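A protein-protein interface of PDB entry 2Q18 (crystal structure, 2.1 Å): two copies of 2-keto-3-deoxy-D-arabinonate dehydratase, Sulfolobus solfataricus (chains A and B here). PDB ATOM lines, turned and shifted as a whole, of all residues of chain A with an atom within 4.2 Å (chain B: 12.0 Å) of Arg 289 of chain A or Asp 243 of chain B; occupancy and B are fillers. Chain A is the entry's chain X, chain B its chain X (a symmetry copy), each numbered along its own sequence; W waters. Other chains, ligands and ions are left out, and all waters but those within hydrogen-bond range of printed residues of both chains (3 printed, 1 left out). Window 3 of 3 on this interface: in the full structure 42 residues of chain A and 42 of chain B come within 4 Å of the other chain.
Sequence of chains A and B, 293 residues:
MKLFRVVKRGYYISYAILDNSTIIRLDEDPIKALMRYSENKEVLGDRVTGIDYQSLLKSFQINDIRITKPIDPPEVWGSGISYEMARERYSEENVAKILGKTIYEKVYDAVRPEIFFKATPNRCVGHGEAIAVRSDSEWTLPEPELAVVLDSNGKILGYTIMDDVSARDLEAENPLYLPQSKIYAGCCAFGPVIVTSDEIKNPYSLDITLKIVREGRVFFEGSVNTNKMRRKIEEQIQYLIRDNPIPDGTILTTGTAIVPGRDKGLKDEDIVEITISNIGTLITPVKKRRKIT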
ATOM      1  N   ALA A 132      18.236 -25.128   5.243  1.00  0.00           N
ATOM      2  CA  ALA A 132      18.617 -24.308   6.384  1.00  0.00           C
ATOM      3  C   ALA A 132      17.429 -23.828   7.202  1.00  0.00           C
ATOM      4  O   ALA A 132      16.311 -23.705   6.692  1.00  0.00           O
ATOM      5  CB  ALA A 132      19.482 -23.126   5.935  1.00  0.00           C
ATOM      6  N   VAL A 133      17.688 -23.594   8.489  1.00  0.00           N
ATOM      7  CA  VAL A 133      16.745 -22.955   9.396  1.00  0.00           C
ATOM      8  C   VAL A 133      17.372 -21.615   9.721  1.00  0.00           C
ATOM      9  O   VAL A 133      18.540 -21.560  10.118  1.00  0.00           O
ATOM     10  CB  VAL A 133      16.533 -23.784  10.706  1.00  0.00           C
ATOM     11  CG1 VAL A 133      15.669 -23.025  11.706  1.00  0.00           C
ATOM     12  CG2 VAL A 133      15.904 -25.136  10.397  1.00  0.00           C
ATOM     13  N   ARG A 134      16.611 -20.538   9.533  1.00  0.00           N
ATOM     14  CA  ARG A 134      17.085 -19.190   9.838  1.00  0.00           C
ATOM     15  C   ARG A 134      17.561 -19.106  11.290  1.00  0.00           C
ATOM     16  O   ARG A 134      16.987 -19.746  12.175  1.00  0.00           O
ATOM     17  CB  ARG A 134      15.965 -18.164   9.606  1.00  0.00           C
ATOM     18  CG  ARG A 134      15.565 -17.935   8.138  1.00  0.00           C
ATOM     19  CD  ARG A 134      14.434 -16.894   8.029  1.00  0.00           C
ATOM     20  NE  ARG A 134      14.826 -15.652   8.690  1.00  0.00           N
ATOM     21  CZ  ARG A 134      15.176 -14.532   8.069  1.00  0.00           C
ATOM     22  NH1 ARG A 134      15.138 -14.445   6.740  1.00  0.00           N
ATOM     23  NH2 ARG A 134      15.540 -13.481   8.791  1.00  0.00           N
ATOM     24  N   SER A 135      18.605 -18.313  11.520  1.00  0.00           N
ATOM     25  CA  SER A 135      19.153 -18.082  12.852  1.00  0.00           C
ATOM     26  C   SER A 135      18.131 -17.483  13.819  1.00  0.00           C
ATOM     27  O   SER A 135      18.247 -17.655  15.036  1.00  0.00           O
ATOM     28  CB  SER A 135      20.372 -17.165  12.768  1.00  0.00           C
ATOM     29  OG  SER A 135      20.013 -15.894  12.250  1.00  0.00           O
ATOM     30  N   TYR A 184      15.604 -17.170   1.676  1.00  0.00           N
ATOM     31  CA  TYR A 184      16.909 -17.105   2.341  1.00  0.00           C
ATOM     32  C   TYR A 184      17.791 -18.259   1.844  1.00  0.00           C
ATOM     33  O   TYR A 184      17.306 -19.147   1.142  1.00  0.00           O
ATOM     34  CB  TYR A 184      16.746 -17.135   3.874  1.00  0.00           C
ATOM     35  CG  TYR A 184      16.009 -18.350   4.400  1.00  0.00           C
ATOM     36  CD1 TYR A 184      16.706 -19.499   4.776  1.00  0.00           C
ATOM     37  CD2 TYR A 184      14.619 -18.353   4.527  1.00  0.00           C
ATOM     38  CE1 TYR A 184      16.038 -20.625   5.252  1.00  0.00           C
ATOM     39  CE2 TYR A 184      13.941 -19.475   5.007  1.00  0.00           C
ATOM     40  CZ  TYR A 184      14.663 -20.604   5.369  1.00  0.00           C
ATOM     41  OH  TYR A 184      14.018 -21.723   5.849  1.00  0.00           O
ATOM     42  N   ALA A 185      19.079 -18.244   2.186  1.00  0.00           N
ATOM     43  CA  ALA A 185      19.990 -19.298   1.735  1.00  0.00           C
ATOM     44  C   ALA A 185      19.539 -20.653   2.270  1.00  0.00           C
ATOM     45  O   ALA A 185      19.381 -20.826   3.478  1.00  0.00           O
ATOM     46  CB  ALA A 185      21.425 -19.000   2.163  1.00  0.00           C
ATOM     47  N   LYS A 287      20.671 -27.720   8.432  1.00  0.00           N
ATOM     48  CA  LYS A 287      21.653 -26.905   9.121  1.00  0.00           C
ATOM     49  C   LYS A 287      20.957 -25.695   9.743  1.00  0.00           C
ATOM     50  O   LYS A 287      20.282 -24.929   9.049  1.00  0.00           O
ATOM     51  CB  LYS A 287      22.764 -26.469   8.155  1.00  0.00           C
ATOM     52  CG  LYS A 287      23.729 -25.419   8.700  1.00  0.00           C
ATOM     53  CD  LYS A 287      24.710 -26.015   9.709  1.00  0.00           C
ATOM     54  CE  LYS A 287      25.505 -24.933  10.429  1.00  0.00           C
ATOM     55  NZ  LYS A 287      26.382 -25.524  11.478  1.00  0.00           N
ATOM     56  N   LYS A 288      21.104 -25.542  11.056  1.00  0.00           N
ATOM     57  CA  LYS A 288      20.621 -24.354  11.741  1.00  0.00           C
ATOM     58  C   LYS A 288      21.653 -23.239  11.595  1.00  0.00           C
ATOM     59  O   LYS A 288      22.820 -23.416  11.950  1.00  0.00           O
ATOM     60  CB  LYS A 288      20.346 -24.651  13.220  1.00  0.00           C
ATOM     61  CG  LYS A 288      20.102 -23.414  14.084  1.00  0.00           C
ATOM     62  CD  LYS A 288      18.685 -22.881  13.935  1.00  0.00           C
ATOM     63  CE  LYS A 288      18.466 -21.662  14.826  1.00  0.00           C
ATOM     64  NZ  LYS A 288      17.027 -21.277  14.884  1.00  0.00           N
ATOM     65  N   ARG A 289      21.218 -22.097  11.066  1.00  0.00           N
ATOM     66  CA  ARG A 289      22.107 -20.953  10.880  1.00  0.00           C
ATOM     67  C   ARG A 289      22.462 -20.305  12.218  1.00  0.00           C
ATOM     68  O   ARG A 289      21.631 -20.232  13.120  1.00  0.00           O
ATOM     69  CB  ARG A 289      21.488 -19.914   9.934  1.00  0.00           C
ATOM     70  CG  ARG A 289      21.186 -20.414   8.519  1.00  0.00           C
ATOM     71  CD  ARG A 289      22.444 -20.762   7.730  1.00  0.00           C
ATOM     72  NE  ARG A 289      22.168 -20.871   6.294  1.00  0.00           N
ATOM     73  CZ  ARG A 289      22.804 -21.687   5.454  1.00  0.00           C
ATOM     74  NH1 ARG A 289      22.472 -21.702   4.170  1.00  0.00           N
ATOM     75  NH2 ARG A 289      23.760 -22.501   5.889  1.00  0.00           N
ATOM     76  N   ARG A 290      23.705 -19.845  12.322  1.00  0.00           N
ATOM     77  CA  ARG A 290      24.229 -19.214  13.531  1.00  0.00           C
ATOM     78  C   ARG A 290      24.044 -17.695  13.470  1.00  0.00           C
ATOM     79  O   ARG A 290      24.180 -17.089  12.403  1.00  0.00           O
ATOM     80  CB  ARG A 290      25.713 -19.573  13.694  1.00  0.00           C
ATOM     81  CG  ARG A 290      26.430 -18.901  14.864  1.00  0.00           C
ATOM     82  CD  ARG A 290      27.938 -19.156  14.823  1.00  0.00           C
ATOM     83  NE  ARG A 290      28.664 -18.318  15.780  1.00  0.00           N
ATOM     84  CZ  ARG A 290      28.868 -18.628  17.060  1.00  0.00           C
ATOM     85  NH1 ARG A 290      28.404 -19.768  17.564  1.00  0.00           N
ATOM     86  NH2 ARG A 290      29.540 -17.793  17.844  1.00  0.00           N
ATOM     87  N   LYS A 291      23.734 -17.092  14.616  1.00  0.00           N
ATOM     88  CA  LYS A 291      23.562 -15.640  14.719  1.00  0.00           C
ATOM     89  C   LYS A 291      24.883 -14.884  14.568  1.00  0.00           C
ATOM     90  O   LYS A 291      25.960 -15.426  14.832  1.00  0.00           O
ATOM     91  CB  LYS A 291      22.891 -15.270  16.047  1.00  0.00           C
ATOM     92  CG  LYS A 291      21.461 -15.777  16.178  1.00  0.00           C
ATOM     93  CD  LYS A 291      20.791 -15.261  17.442  1.00  0.00           C
ATOM     94  CE  LYS A 291      19.342 -15.723  17.517  1.00  0.00           C
ATOM     95  NZ  LYS A 291      18.623 -15.151  18.693  1.00  0.00           N
ATOM     96  N   GLU B  75      19.060  -8.288  -8.029  1.00  0.00           N
ATOM     97  CA  GLU B  75      17.867  -8.435  -7.202  1.00  0.00           C
ATOM     98  C   GLU B  75      17.383  -7.070  -6.764  1.00  0.00           C
ATOM     99  O   GLU B  75      18.187  -6.161  -6.543  1.00  0.00           O
ATOM    100  CB  GLU B  75      18.150  -9.305  -5.963  1.00  0.00           C
ATOM    101  CG  GLU B  75      18.547 -10.736  -6.301  1.00  0.00           C
ATOM    102  CD  GLU B  75      18.800 -11.614  -5.077  1.00  0.00           C
ATOM    103  OE1 GLU B  75      18.532 -11.182  -3.932  1.00  0.00           O
ATOM    104  OE2 GLU B  75      19.266 -12.751  -5.278  1.00  0.00           O
ATOM    105  N   TRP B  77      14.821  -5.518  -3.761  1.00  0.00           N
ATOM    106  CA  TRP B  77      14.043  -5.769  -2.561  1.00  0.00           C
ATOM    107  C   TRP B  77      13.443  -4.455  -2.067  1.00  0.00           C
ATOM    108  O   TRP B  77      13.956  -3.371  -2.358  1.00  0.00           O
ATOM    109  CB  TRP B  77      14.930  -6.369  -1.465  1.00  0.00           C
ATOM    110  CG  TRP B  77      15.412  -7.771  -1.743  1.00  0.00           C
ATOM    111  CD1 TRP B  77      16.414  -8.145  -2.594  1.00  0.00           C
ATOM    112  CD2 TRP B  77      14.921  -8.979  -1.147  1.00  0.00           C
ATOM    113  NE1 TRP B  77      16.578  -9.513  -2.565  1.00  0.00           N
ATOM    114  CE2 TRP B  77      15.674 -10.049  -1.685  1.00  0.00           C
ATOM    115  CE3 TRP B  77      13.924  -9.260  -0.199  1.00  0.00           C
ATOM    116  CZ2 TRP B  77      15.456 -11.382  -1.315  1.00  0.00           C
ATOM    117  CZ3 TRP B  77      13.705 -10.584   0.167  1.00  0.00           C
ATOM    118  CH2 TRP B  77      14.473 -11.628  -0.389  1.00  0.00           C
ATOM    119  N   ARG B 112      11.045  -6.177  14.150  1.00  0.00           N
ATOM    120  CA  ARG B 112      11.302  -6.677  12.796  1.00  0.00           C
ATOM    121  C   ARG B 112      10.568  -5.846  11.737  1.00  0.00           C
ATOM    122  O   ARG B 112       9.335  -5.806  11.726  1.00  0.00           O
ATOM    123  CB  ARG B 112      10.900  -8.155  12.672  1.00  0.00           C
ATOM    124  CG  ARG B 112      11.204  -8.768  11.297  1.00  0.00           C
ATOM    125  CD  ARG B 112      10.757 -10.224  11.192  1.00  0.00           C
ATOM    126  NE  ARG B 112      11.420 -11.071  12.185  1.00  0.00           N
ATOM    127  CZ  ARG B 112      12.624 -11.621  12.041  1.00  0.00           C
ATOM    128  NH1 ARG B 112      13.125 -12.370  13.017  1.00  0.00           N
ATOM    129  NH2 ARG B 112      13.329 -11.433  10.931  1.00  0.00           N
ATOM    130  N   ILE B 115      10.254  -6.655   4.985  1.00  0.00           N
ATOM    131  CA  ILE B 115      11.190  -6.815   3.868  1.00  0.00           C
ATOM    132  C   ILE B 115      10.531  -7.745   2.856  1.00  0.00           C
ATOM    133  O   ILE B 115      10.072  -8.830   3.219  1.00  0.00           O
ATOM    134  CB  ILE B 115      12.542  -7.443   4.337  1.00  0.00           C
ATOM    135  CG1 ILE B 115      13.302  -6.521   5.308  1.00  0.00           C
ATOM    136  CG2 ILE B 115      13.424  -7.855   3.144  1.00  0.00           C
ATOM    137  CD1 ILE B 115      13.834  -5.217   4.710  1.00  0.00           C
ATOM    138  N   SER B 152      27.609  -7.157  -1.740  1.00  0.00           N
ATOM    139  CA  SER B 152      27.212  -8.407  -1.073  1.00  0.00           C
ATOM    140  C   SER B 152      27.327  -8.381   0.461  1.00  0.00           C
ATOM    141  O   SER B 152      26.716  -9.205   1.135  1.00  0.00           O
ATOM    142  CB  SER B 152      27.963  -9.612  -1.662  1.00  0.00           C
ATOM    143  OG  SER B 152      29.362  -9.434  -1.571  1.00  0.00           O
ATOM    144  N   ASN B 153      28.089  -7.427   0.998  1.00  0.00           N
ATOM    145  CA  ASN B 153      28.192  -7.229   2.447  1.00  0.00           C
ATOM    146  C   ASN B 153      27.144  -6.276   3.014  1.00  0.00           C
ATOM    147  O   ASN B 153      27.099  -6.039   4.225  1.00  0.00           O
ATOM    148  CB  ASN B 153      29.584  -6.716   2.832  1.00  0.00           C
ATOM    149  CG  ASN B 153      30.684  -7.683   2.467  1.00  0.00           C
ATOM    150  OD1 ASN B 153      31.764  -7.271   2.044  1.00  0.00           O
ATOM    151  ND2 ASN B 153      30.416  -8.976   2.614  1.00  0.00           N
ATOM    152  N   GLY B 154      26.312  -5.720   2.139  1.00  0.00           N
ATOM    153  CA  GLY B 154      25.287  -4.777   2.563  1.00  0.00           C
ATOM    154  C   GLY B 154      25.801  -3.358   2.702  1.00  0.00           C
ATOM    155  O   GLY B 154      25.125  -2.505   3.278  1.00  0.00           O
ATOM    156  N   GLU B 235      19.141  -0.554   9.435  1.00  0.00           N
ATOM    157  CA  GLU B 235      18.325  -1.624  10.001  1.00  0.00           C
ATOM    158  C   GLU B 235      17.627  -2.436   8.911  1.00  0.00           C
ATOM    159  O   GLU B 235      17.504  -3.661   9.024  1.00  0.00           O
ATOM    160  CB  GLU B 235      17.294  -1.054  10.979  1.00  0.00           C
ATOM    161  CG  GLU B 235      16.513  -2.114  11.751  1.00  0.00           C
ATOM    162  CD  GLU B 235      15.435  -1.529  12.654  1.00  0.00           C
ATOM    163  OE1 GLU B 235      15.554  -0.352  13.068  1.00  0.00           O
ATOM    164  OE2 GLU B 235      14.460  -2.254  12.952  1.00  0.00           O
ATOM    165  N   GLN B 236      17.167  -1.752   7.863  1.00  0.00           N
ATOM    166  CA  GLN B 236      16.534  -2.429   6.732  1.00  0.00           C
ATOM    167  C   GLN B 236      17.525  -3.387   6.071  1.00  0.00           C
ATOM    168  O   GLN B 236      17.175  -4.526   5.760  1.00  0.00           O
ATOM    169  CB  GLN B 236      16.006  -1.425   5.704  1.00  0.00           C
ATOM    170  CG  GLN B 236      14.969  -0.437   6.246  1.00  0.00           C
ATOM    171  CD  GLN B 236      14.417   0.478   5.162  1.00  0.00           C
ATOM    172  OE1 GLN B 236      14.660   0.266   3.971  1.00  0.00           O
ATOM    173  NE2 GLN B 236      13.667   1.493   5.569  1.00  0.00           N
ATOM    174  N   ILE B 237      18.756  -2.916   5.873  1.00  0.00           N
ATOM    175  CA  ILE B 237      19.823  -3.731   5.287  1.00  0.00           C
ATOM    176  C   ILE B 237      20.139  -4.939   6.178  1.00  0.00           C
ATOM    177  O   ILE B 237      20.258  -6.060   5.679  1.00  0.00           O
ATOM    178  CB  ILE B 237      21.110  -2.909   5.016  1.00  0.00           C
ATOM    179  CG1 ILE B 237      20.831  -1.780   4.013  1.00  0.00           C
ATOM    180  CG2 ILE B 237      22.235  -3.817   4.503  1.00  0.00           C
ATOM    181  CD1 ILE B 237      21.973  -0.789   3.857  1.00  0.00           C
ATOM    182  N   GLN B 238      20.252  -4.700   7.487  1.00  0.00           N
ATOM    183  CA  GLN B 238      20.484  -5.766   8.474  1.00  0.00           C
ATOM    184  C   GLN B 238      19.515  -6.939   8.298  1.00  0.00           C
ATOM    185  O   GLN B 238      19.938  -8.086   8.200  1.00  0.00           O
ATOM    186  CB  GLN B 238      20.406  -5.207   9.906  1.00  0.00           C
ATOM    187  CG  GLN B 238      20.505  -6.265  11.012  1.00  0.00           C
ATOM    188  CD  GLN B 238      20.226  -5.728  12.423  1.00  0.00           C
ATOM    189  OE1 GLN B 238      20.261  -6.484  13.393  1.00  0.00           O
ATOM    190  NE2 GLN B 238      19.951  -4.430  12.539  1.00  0.00           N
ATOM    191  N   TYR B 239      18.219  -6.646   8.245  1.00  0.00           N
ATOM    192  CA  TYR B 239      17.207  -7.695   8.114  1.00  0.00           C
ATOM    193  C   TYR B 239      17.131  -8.295   6.706  1.00  0.00           C
ATOM    194  O   TYR B 239      16.747  -9.456   6.547  1.00  0.00           O
ATOM    195  CB  TYR B 239      15.836  -7.198   8.589  1.00  0.00           C
ATOM    196  CG  TYR B 239      15.711  -7.164  10.099  1.00  0.00           C
ATOM    197  CD1 TYR B 239      16.223  -6.096  10.840  1.00  0.00           C
ATOM    198  CD2 TYR B 239      15.100  -8.212  10.789  1.00  0.00           C
ATOM    199  CE1 TYR B 239      16.117  -6.070  12.234  1.00  0.00           C
ATOM    200  CE2 TYR B 239      14.990  -8.196  12.182  1.00  0.00           C
ATOM    201  CZ  TYR B 239      15.500  -7.124  12.894  1.00  0.00           C
ATOM    202  OH  TYR B 239      15.395  -7.109  14.267  1.00  0.00           O
ATOM    203  N   LEU B 240      17.499  -7.505   5.697  1.00  0.00           N
ATOM    204  CA  LEU B 240      17.565  -7.994   4.317  1.00  0.00           C
ATOM    205  C   LEU B 240      18.605  -9.107   4.161  1.00  0.00           C
ATOM    206  O   LEU B 240      18.310 -10.161   3.594  1.00  0.00           O
ATOM    207  CB  LEU B 240      17.874  -6.851   3.336  1.00  0.00           C
ATOM    208  CG  LEU B 240      18.221  -7.258   1.892  1.00  0.00           C
ATOM    209  CD1 LEU B 240      17.075  -8.025   1.243  1.00  0.00           C
ATOM    210  CD2 LEU B 240      18.612  -6.052   1.042  1.00  0.00           C
ATOM    211  N   ILE B 241      19.813  -8.863   4.666  1.00  0.00           N
ATOM    212  CA  ILE B 241      20.943  -9.768   4.434  1.00  0.00           C
ATOM    213  C   ILE B 241      21.055 -10.914   5.443  1.00  0.00           C
ATOM    214  O   ILE B 241      21.862 -11.830   5.251  1.00  0.00           O
ATOM    215  CB  ILE B 241      22.295  -9.002   4.315  1.00  0.00           C
ATOM    216  CG1 ILE B 241      22.710  -8.389   5.662  1.00  0.00           C
ATOM    217  CG2 ILE B 241      22.212  -7.947   3.209  1.00  0.00           C
ATOM    218  CD1 ILE B 241      24.127  -7.820   5.680  1.00  0.00           C
ATOM    219  N   ARG B 242      20.240 -10.875   6.497  1.00  0.00           N
ATOM    220  CA  ARG B 242      20.262 -11.919   7.527  1.00  0.00           C
ATOM    221  C   ARG B 242      19.934 -13.291   6.948  1.00  0.00           C
ATOM    222  O   ARG B 242      18.817 -13.517   6.476  1.00  0.00           O
ATOM    223  CB  ARG B 242      19.295 -11.592   8.668  1.00  0.00           C
ATOM    224  CG  ARG B 242      19.302 -12.635   9.783  1.00  0.00           C
ATOM    225  CD  ARG B 242      18.361 -12.266  10.906  1.00  0.00           C
ATOM    226  NE  ARG B 242      18.842 -11.120  11.678  1.00  0.00           N
ATOM    227  CZ  ARG B 242      18.197 -10.600  12.719  1.00  0.00           C
ATOM    228  NH1 ARG B 242      17.039 -11.118  13.115  1.00  0.00           N
ATOM    229  NH2 ARG B 242      18.708  -9.560  13.361  1.00  0.00           N
ATOM    230  N   ASP B 243      20.919 -14.192   6.992  1.00  0.00           N
ATOM    231  CA  ASP B 243      20.800 -15.552   6.450  1.00  0.00           C
ATOM    232  C   ASP B 243      20.397 -15.564   4.970  1.00  0.00           C
ATOM    233  O   ASP B 243      19.894 -16.566   4.455  1.00  0.00           O
ATOM    234  CB  ASP B 243      19.828 -16.389   7.294  1.00  0.00           C
ATOM    235  CG  ASP B 243      20.266 -16.502   8.749  1.00  0.00           C
ATOM    236  OD1 ASP B 243      21.488 -16.564   9.006  1.00  0.00           O
ATOM    237  OD2 ASP B 243      19.387 -16.527   9.633  1.00  0.00           O
ATOM    238  N   ASN B 244      20.645 -14.444   4.298  1.00  0.00           N
ATOM    239  CA  ASN B 244      20.114 -14.202   2.962  1.00  0.00           C
ATOM    240  C   ASN B 244      21.137 -13.454   2.114  1.00  0.00           C
ATOM    241  O   ASN B 244      21.188 -12.228   2.138  1.00  0.00           O
ATOM    242  CB  ASN B 244      18.798 -13.418   3.061  1.00  0.00           C
ATOM    243  CG  ASN B 244      18.101 -13.257   1.719  1.00  0.00           C
ATOM    244  OD1 ASN B 244      18.146 -14.147   0.864  1.00  0.00           O
ATOM    245  ND2 ASN B 244      17.434 -12.117   1.536  1.00  0.00           N
ATOM    246  N   PRO B 245      21.970 -14.199   1.370  1.00  0.00           N
ATOM    247  CA  PRO B 245      23.016 -13.565   0.574  1.00  0.00           C
ATOM    248  C   PRO B 245      22.417 -12.750  -0.564  1.00  0.00           C
ATOM    249  O   PRO B 245      21.456 -13.181  -1.199  1.00  0.00           O
ATOM    250  CB  PRO B 245      23.814 -14.754   0.019  1.00  0.00           C
ATOM    251  CG  PRO B 245      22.856 -15.899   0.030  1.00  0.00           C
ATOM    252  CD  PRO B 245      21.974 -15.666   1.226  1.00  0.00           C
ATOM    253  N   ILE B 246      22.975 -11.568  -0.795  1.00  0.00           N
ATOM    254  CA  ILE B 246      22.561 -10.729  -1.914  1.00  0.00           C
ATOM    255  C   ILE B 246      23.761 -10.460  -2.821  1.00  0.00           C
ATOM    256  O   ILE B 246      24.880 -10.318  -2.336  1.00  0.00           O
ATOM    257  CB  ILE B 246      21.903  -9.401  -1.439  1.00  0.00           C
ATOM    258  CG1 ILE B 246      22.833  -8.634  -0.490  1.00  0.00           C
ATOM    259  CG2 ILE B 246      20.541  -9.686  -0.781  1.00  0.00           C
ATOM    260  CD1 ILE B 246      22.547  -7.143  -0.392  1.00  0.00           C
ATOM    261  N   PRO B 247      23.539 -10.428  -4.146  1.00  0.00           N
ATOM    262  CA  PRO B 247      24.634 -10.117  -5.067  1.00  0.00           C
ATOM    263  C   PRO B 247      25.009  -8.638  -5.086  1.00  0.00           C
ATOM    264  O   PRO B 247      24.213  -7.790  -4.668  1.00  0.00           O
ATOM    265  CB  PRO B 247      24.082 -10.550  -6.429  1.00  0.00           C
ATOM    266  CG  PRO B 247      22.605 -10.497  -6.279  1.00  0.00           C
ATOM    267  CD  PRO B 247      22.277 -10.739  -4.849  1.00  0.00           C
HETATM  268  O   HOH W   1      22.803 -15.080  10.801  1.00  0.00           O
HETATM  269  O   HOH W   2      20.211 -19.311   5.423  1.00  0.00           O
HETATM  270  O   HOH W   3      15.399 -10.934   8.283  1.00  0.00           O
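The backbone NH (N) of Ala 185 of chain A lies within hydrogen-bond range of the backbone carbonyl oxygen (O) of Asp 243 of chain B (2.9 Å). OD2 of Asp 243 of chain B is in hydrogen-bond range of N of Ser 135 of chain A.
The backbone carbonyl oxygen (O) of Ala 185 of chain A sits at hydrogen-bond distance from the guanidinium group (NH1) of Arg 289 of chain A, 3.3 Å away. The backbone carbonyl oxygen (O) of Ala 132 of chain A is in hydrogen-bond range of the side-chain hydroxyl (OH) of Tyr 184 of chain A, at 3.1 Å. The backbone carbonyl oxygen of Val 133 of chain A is in hydrogen-bond range of the backbone NH of Arg 289 of chain A (2.9 Å). NZ of Lys 288 of chain A is in hydrogen-bond range of O of Arg 134 of chain A. The backbone carbonyl oxygen (O) of Leu 240 of chain B sits at hydrogen-bond distance from the side-chain amide nitrogen (ND2) of Asn 244 of chain B. NH2 of Arg 242 of chain B is in hydrogen-bond range of OE1 of Gln 238 of chain B (3.4 Å).
Among the printed residues, pairs that only touch across the chains: Arg 134 of chain A with Arg 112 of chain B, Arg 134 of chain A with Arg 242 of chain B, Arg 134 of chain A with Asp 243 of chain B, Tyr 184 of chain A with Asp 243 of chain B, Tyr 184 of chain A with Asn 244 of chain B, Ala 185 of chain A with Pro 245 of chain B and Arg 289 of chain A with Asp 243 of chain B.
Arg 289 of chain A touches one residue of chain B. Asp 243 of chain B touches just these residues of chain A: Arg 134 (3.5 Å), Ser 135 (2.7 Å), Tyr 184 (3.3 Å), Ala 185 (2.9 Å) and Arg 289 (3.5 Å). No residue of chain B comes within 4 Å of Ala 132 of chain A. No residue of chain B comes within 4 Å of Val 133 of chain A. Arg 134 of chain A touches just these residues of chain B: Arg 112, Arg 242 and Asp 243. Ser 135 of chain A touches one residue of chain B. Printed residues of chain B within 4 Å of Tyr 184 of chain A: Asp 243 and Asn 244. No residue of chain B comes within 4 Å of Lys 287 of chain A. Printed residues of chain A within 4 Å of Arg 112 of chain B: Arg 134. Printed residues of chain A within 4 Å of Arg 242 of chain B: Arg 134. Printed residues of chain A within 4 Å of Pro 245 of chain B: Ala 185 (3.5 Å). Of the printed residues of chain A, Asn 244 of chain B touches Tyr 184 (3.5 Å). Glu 75 of chain B touches none of the printed residues of chain A. The nearest printed residue of chain A that does not touch Asp 243 of chain B is Arg 290 of chain A (4.4 Å).
Hydrophobic or aromatic side chains of chain B that line the printed part of chain A: Pro 245.
No position is printed for both chains.
Water W3 lies within hydrogen-bond range of the guanidinium group of Arg 134 of chain A, the backbone carbonyl oxygen of Tyr 239 of chain B and the guanidinium group of Arg 112 of chain B. Water W2 lies within hydrogen-bond range of O of Ala 185 of chain A (2.6 Å), NE of Arg 289 of chain A (2.6 Å) and O of Asp 243 of chain B (2.9 Å). Water W1 lies within hydrogen-bond range of the side-chain carboxylate of Asp 243 of chain B (2.7 Å), the backbone carbonyl oxygen of Arg 290 of chain A (2.9 Å) and the side-chain hydroxyl of Ser 135 of chain A (3.2 Å).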
